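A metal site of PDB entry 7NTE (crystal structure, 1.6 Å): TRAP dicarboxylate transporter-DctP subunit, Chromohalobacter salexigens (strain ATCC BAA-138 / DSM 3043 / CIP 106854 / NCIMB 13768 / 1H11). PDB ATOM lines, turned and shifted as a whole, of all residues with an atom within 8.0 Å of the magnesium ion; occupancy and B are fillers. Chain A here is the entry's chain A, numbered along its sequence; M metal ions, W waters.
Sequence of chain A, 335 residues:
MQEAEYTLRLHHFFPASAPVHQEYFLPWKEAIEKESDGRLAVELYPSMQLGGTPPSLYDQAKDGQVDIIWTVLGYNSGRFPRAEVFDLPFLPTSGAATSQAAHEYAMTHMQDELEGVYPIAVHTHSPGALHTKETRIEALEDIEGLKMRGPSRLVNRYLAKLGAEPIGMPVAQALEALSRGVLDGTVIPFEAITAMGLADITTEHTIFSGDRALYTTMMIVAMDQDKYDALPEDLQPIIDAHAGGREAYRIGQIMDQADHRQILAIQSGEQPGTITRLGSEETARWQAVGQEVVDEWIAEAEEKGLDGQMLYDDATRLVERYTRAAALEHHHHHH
The backbone carbonyl oxygen of Glu 115 lies close to the side-chain amino group of Lys 62, at 3.3 Å.
The nearest printed residue that does not touch the magnesium ion is Asp 63 (4.2 Å).
The magnesium ion is bound by water W2 (2.0 Å), OD2 of Asp 226 (2.0 Å), O of Lys 62 (2.0 Å), OD1 of Asp 224 (2.1 Å), water W3 (2.2 Å) and water W1 (2.2 Å).
Water W1 bridges OD2 of Asp 224 (2.6 Å) and N of Gly 64 (3.5 Å).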
ATOM      1  N   TYR A  58      21.021 -15.015 -19.166  1.00  0.00           N
ATOM      2  CA  TYR A  58      20.977 -14.339 -20.452  1.00  0.00           C
ATOM      3  C   TYR A  58      22.174 -13.418 -20.596  1.00  0.00           C
ATOM      4  O   TYR A  58      22.859 -13.448 -21.624  1.00  0.00           O
ATOM      5  CB  TYR A  58      19.671 -13.553 -20.623  1.00  0.00           C
ATOM      6  CG  TYR A  58      19.472 -12.922 -21.962  1.00  0.00           C
ATOM      7  CD1 TYR A  58      18.977 -13.679 -23.048  1.00  0.00           C
ATOM      8  CD2 TYR A  58      19.765 -11.586 -22.163  1.00  0.00           C
ATOM      9  CE1 TYR A  58      18.799 -13.090 -24.286  1.00  0.00           C
ATOM     10  CE2 TYR A  58      19.557 -10.992 -23.387  1.00  0.00           C
ATOM     11  CZ  TYR A  58      19.096 -11.744 -24.451  1.00  0.00           C
ATOM     12  OH  TYR A  58      18.926 -11.138 -25.664  1.00  0.00           O
ATOM     13  N   ASP A  59      22.418 -12.663 -19.540  1.00  0.00           N
ATOM     14  CA  ASP A  59      23.576 -11.780 -19.516  1.00  0.00           C
ATOM     15  C   ASP A  59      24.891 -12.513 -19.430  1.00  0.00           C
ATOM     16  O   ASP A  59      25.924 -12.004 -19.905  1.00  0.00           O
ATOM     17  CB  ASP A  59      23.414 -10.734 -18.406  1.00  0.00           C
ATOM     18  CG  ASP A  59      22.282  -9.760 -18.711  1.00  0.00           C
ATOM     19  OD1 ASP A  59      22.328  -9.100 -19.774  1.00  0.00           O
ATOM     20  OD2 ASP A  59      21.368  -9.669 -17.878  1.00  0.00           O
ATOM     21  N   GLN A  60      24.931 -13.699 -18.827  1.00  0.00           N
ATOM     22  CA  GLN A  60      26.194 -14.459 -18.832  1.00  0.00           C
ATOM     23  C   GLN A  60      26.664 -14.725 -20.246  1.00  0.00           C
ATOM     24  O   GLN A  60      27.836 -14.621 -20.547  1.00  0.00           O
ATOM     25  CB  GLN A  60      26.079 -15.744 -18.049  1.00  0.00           C
ATOM     26  CG  GLN A  60      25.957 -15.568 -16.546  1.00  0.00           C
ATOM     27  CD  GLN A  60      25.921 -16.911 -15.847  1.00  0.00           C
ATOM     28  OE1 GLN A  60      26.137 -17.928 -16.464  1.00  0.00           O
ATOM     29  NE2 GLN A  60      25.641 -16.905 -14.563  1.00  0.00           N
ATOM     30  N   ALA A  61      25.744 -15.060 -21.151  1.00  0.00           N
ATOM     31  CA  ALA A  61      26.127 -15.302 -22.537  1.00  0.00           C
ATOM     32  C   ALA A  61      26.394 -13.988 -23.261  1.00  0.00           C
ATOM     33  O   ALA A  61      27.418 -13.844 -23.904  1.00  0.00           O
ATOM     34  CB  ALA A  61      25.024 -16.064 -23.245  1.00  0.00           C
ATOM     35  N   LYS A  62      25.493 -13.016 -23.136  1.00  0.00           N
ATOM     36  CA  LYS A  62      25.644 -11.754 -23.843  1.00  0.00           C
ATOM     37  C   LYS A  62      26.995 -11.112 -23.470  1.00  0.00           C
ATOM     38  O   LYS A  62      27.683 -10.609 -24.351  1.00  0.00           O
ATOM     39  CB  LYS A  62      24.432 -10.845 -23.566  1.00  0.00           C
ATOM     40  CG  LYS A  62      24.342  -9.630 -24.443  1.00  0.00           C
ATOM     41  CD  LYS A  62      22.968  -8.970 -24.265  1.00  0.00           C
ATOM     42  CE  LYS A  62      22.916  -7.688 -25.054  1.00  0.00           C
ATOM     43  NZ  LYS A  62      21.627  -7.034 -24.764  1.00  0.00           N
ATOM     44  N   ASP A  63      27.370 -11.158 -22.203  1.00  0.00           N
ATOM     45  CA  ASP A  63      28.615 -10.540 -21.688  1.00  0.00           C
ATOM     46  C   ASP A  63      29.873 -11.388 -21.887  1.00  0.00           C
ATOM     47  O   ASP A  63      30.961 -10.909 -21.597  1.00  0.00           O
ATOM     48  CB  ASP A  63      28.527 -10.153 -20.215  1.00  0.00           C
ATOM     49  CG  ASP A  63      27.397  -9.170 -19.895  1.00  0.00           C
ATOM     50  OD1 ASP A  63      26.932  -8.437 -20.791  1.00  0.00           O
ATOM     51  OD2 ASP A  63      26.990  -9.134 -18.698  1.00  0.00           O
ATOM     52  N   GLY A  64      29.740 -12.635 -22.326  1.00  0.00           N
ATOM     53  CA  GLY A  64      30.887 -13.485 -22.624  1.00  0.00           C
ATOM     54  C   GLY A  64      31.506 -14.152 -21.424  1.00  0.00           C
ATOM     55  O   GLY A  64      32.642 -14.657 -21.493  1.00  0.00           O
ATOM     56  N   GLN A  65      30.762 -14.214 -20.319  1.00  0.00           N
ATOM     57  CA  GLN A  65      31.209 -15.022 -19.193  1.00  0.00           C
ATOM     58  C   GLN A  65      31.145 -16.503 -19.488  1.00  0.00           C
ATOM     59  O   GLN A  65      31.991 -17.269 -19.022  1.00  0.00           O
ATOM     60  CB  GLN A  65      30.406 -14.728 -17.966  1.00  0.00           C
ATOM     61  CG  GLN A  65      30.751 -13.349 -17.430  1.00  0.00           C
ATOM     62  CD  GLN A  65      29.817 -12.931 -16.330  1.00  0.00           C
ATOM     63  OE1 GLN A  65      28.598 -12.913 -16.505  1.00  0.00           O
ATOM     64  NE2 GLN A  65      30.381 -12.596 -15.167  1.00  0.00           N
ATOM     65  N   VAL A  66      30.098 -16.882 -20.237  1.00  0.00           N
ATOM     66  CA  VAL A  66      29.977 -18.211 -20.834  1.00  0.00           C
ATOM     67  C   VAL A  66      29.637 -17.995 -22.308  1.00  0.00           C
ATOM     68  O   VAL A  66      29.398 -16.878 -22.731  1.00  0.00           O
ATOM     69  CB  VAL A  66      28.920 -19.094 -20.120  1.00  0.00           C
ATOM     70  CG1 VAL A  66      29.209 -19.223 -18.623  1.00  0.00           C
ATOM     71  CG2 VAL A  66      27.501 -18.594 -20.384  1.00  0.00           C
ATOM     72  N   GLU A 115      19.263  -8.468 -29.457  1.00  0.00           N
ATOM     73  CA  GLU A 115      20.528  -7.919 -29.915  1.00  0.00           C
ATOM     74  C   GLU A 115      21.641  -8.438 -29.001  1.00  0.00           C
ATOM     75  O   GLU A 115      21.478  -8.439 -27.788  1.00  0.00           O
ATOM     76  CB  GLU A 115      20.451  -6.365 -29.907  1.00  0.00           C
ATOM     77  CG  GLU A 115      21.699  -5.563 -29.498  1.00  0.00           C
ATOM     78  CD  GLU A 115      22.802  -5.573 -30.524  1.00  0.00           C
ATOM     79  OE1 GLU A 115      22.509  -5.334 -31.722  1.00  0.00           O
ATOM     80  OE2 GLU A 115      23.972  -5.788 -30.138  1.00  0.00           O
ATOM     81  N   GLY A 116      22.753  -8.874 -29.580  1.00  0.00           N
ATOM     82  CA  GLY A 116      23.856  -9.354 -28.796  1.00  0.00           C
ATOM     83  C   GLY A 116      23.880 -10.837 -28.529  1.00  0.00           C
ATOM     84  O   GLY A 116      24.869 -11.329 -27.942  1.00  0.00           O
ATOM     85  N   VAL A 117      22.826 -11.567 -28.908  1.00  0.00           N
ATOM     86  CA  VAL A 117      22.904 -13.015 -28.872  1.00  0.00           C
ATOM     87  C   VAL A 117      22.608 -13.594 -30.230  1.00  0.00           C
ATOM     88  O   VAL A 117      21.789 -13.034 -30.989  1.00  0.00           O
ATOM     89  CB  VAL A 117      22.035 -13.701 -27.800  1.00  0.00           C
ATOM     90  CG1 VAL A 117      22.324 -13.139 -26.421  1.00  0.00           C
ATOM     91  CG2 VAL A 117      20.548 -13.664 -28.113  1.00  0.00           C
ATOM     92  N   MET A 223      23.633 -17.950 -27.907  1.00  0.00           N
ATOM     93  CA  MET A 223      25.099 -17.898 -27.933  1.00  0.00           C
ATOM     94  C   MET A 223      25.536 -16.426 -27.871  1.00  0.00           C
ATOM     95  O   MET A 223      24.883 -15.554 -28.464  1.00  0.00           O
ATOM     96  CB  MET A 223      25.605 -18.589 -29.200  1.00  0.00           C
ATOM     97  CG  MET A 223      27.099 -18.575 -29.328  1.00  0.00           C
ATOM     98  SD  MET A 223      27.572 -19.631 -30.743  1.00  0.00           S
ATOM     99  CE  MET A 223      29.329 -19.685 -30.508  1.00  0.00           C
ATOM    100  N   ASP A 224      26.623 -16.124 -27.158  1.00  0.00           N
ATOM    101  CA  ASP A 224      27.223 -14.773 -27.238  1.00  0.00           C
ATOM    102  C   ASP A 224      27.465 -14.423 -28.712  1.00  0.00           C
ATOM    103  O   ASP A 224      28.200 -15.144 -29.416  1.00  0.00           O
ATOM    104  CB  ASP A 224      28.554 -14.776 -26.492  1.00  0.00           C
ATOM    105  CG  ASP A 224      29.153 -13.396 -26.315  1.00  0.00           C
ATOM    106  OD1 ASP A 224      28.513 -12.365 -26.658  1.00  0.00           O
ATOM    107  OD2 ASP A 224      30.289 -13.358 -25.776  1.00  0.00           O
ATOM    108  N   GLN A 225      26.857 -13.341 -29.207  1.00  0.00           N
ATOM    109  CA  GLN A 225      27.129 -12.957 -30.583  1.00  0.00           C
ATOM    110  C   GLN A 225      28.623 -12.721 -30.799  1.00  0.00           C
ATOM    111  O   GLN A 225      29.148 -13.013 -31.862  1.00  0.00           O
ATOM    112  CB  GLN A 225      26.376 -11.702 -30.937  1.00  0.00           C
ATOM    113  CG  GLN A 225      26.490 -11.298 -32.399  1.00  0.00           C
ATOM    114  CD  GLN A 225      25.751 -12.243 -33.327  1.00  0.00           C
ATOM    115  OE1 GLN A 225      24.576 -12.560 -33.113  1.00  0.00           O
ATOM    116  NE2 GLN A 225      26.432 -12.706 -34.354  1.00  0.00           N
ATOM    117  N   ASP A 226      29.315 -12.214 -29.777  1.00  0.00           N
ATOM    118  CA  ASP A 226      30.746 -11.953 -29.920  1.00  0.00           C
ATOM    119  C   ASP A 226      31.545 -13.221 -30.126  1.00  0.00           C
ATOM    120  O   ASP A 226      32.514 -13.210 -30.884  1.00  0.00           O
ATOM    121  CB  ASP A 226      31.257 -11.202 -28.697  1.00  0.00           C
ATOM    122  CG  ASP A 226      30.601  -9.844 -28.544  1.00  0.00           C
ATOM    123  OD1 ASP A 226      31.092  -8.869 -29.139  1.00  0.00           O
ATOM    124  OD2 ASP A 226      29.566  -9.767 -27.858  1.00  0.00           O
ATOM    125  N   LYS A 227      31.128 -14.312 -29.505  1.00  0.00           N
ATOM    126  CA  LYS A 227      31.834 -15.572 -29.660  1.00  0.00           C
ATOM    127  C   LYS A 227      31.599 -16.183 -31.032  1.00  0.00           C
ATOM    128  O   LYS A 227      32.532 -16.664 -31.644  1.00  0.00           O
ATOM    129  CB  LYS A 227      31.478 -16.550 -28.573  1.00  0.00           C
ATOM    130  CG  LYS A 227      32.318 -17.830 -28.621  1.00  0.00           C
ATOM    131  CD  LYS A 227      33.811 -17.547 -28.393  1.00  0.00           C
ATOM    132  CE  LYS A 227      34.517 -18.805 -27.865  1.00  0.00           C
ATOM    133  NZ  LYS A 227      35.852 -18.535 -27.257  1.00  0.00           N
ATOM    134  N   ASP A 229      30.906 -14.421 -33.659  1.00  0.00           N
ATOM    135  CA  ASP A 229      31.647 -13.535 -34.564  1.00  0.00           C
ATOM    136  C   ASP A 229      33.147 -13.813 -34.547  1.00  0.00           C
ATOM    137  O   ASP A 229      33.811 -13.566 -35.536  1.00  0.00           O
ATOM    138  CB  ASP A 229      31.390 -12.054 -34.211  1.00  0.00           C
ATOM    139  CG  ASP A 229      29.978 -11.590 -34.527  1.00  0.00           C
ATOM    140  OD1 ASP A 229      29.236 -12.286 -35.269  1.00  0.00           O
ATOM    141  OD2 ASP A 229      29.612 -10.500 -34.035  1.00  0.00           O
HETATM  142 MG    MG M   1      28.611 -10.331 -26.147  1.00  0.00          MG
HETATM  143  O   HOH W   1      30.515 -10.824 -25.172  1.00  0.00           O
HETATM  144  O   HOH W   2      26.933  -9.806 -27.078  1.00  0.00           O
HETATM  145  O   HOH W   3      28.815  -8.287 -25.434  1.00  0.00           O
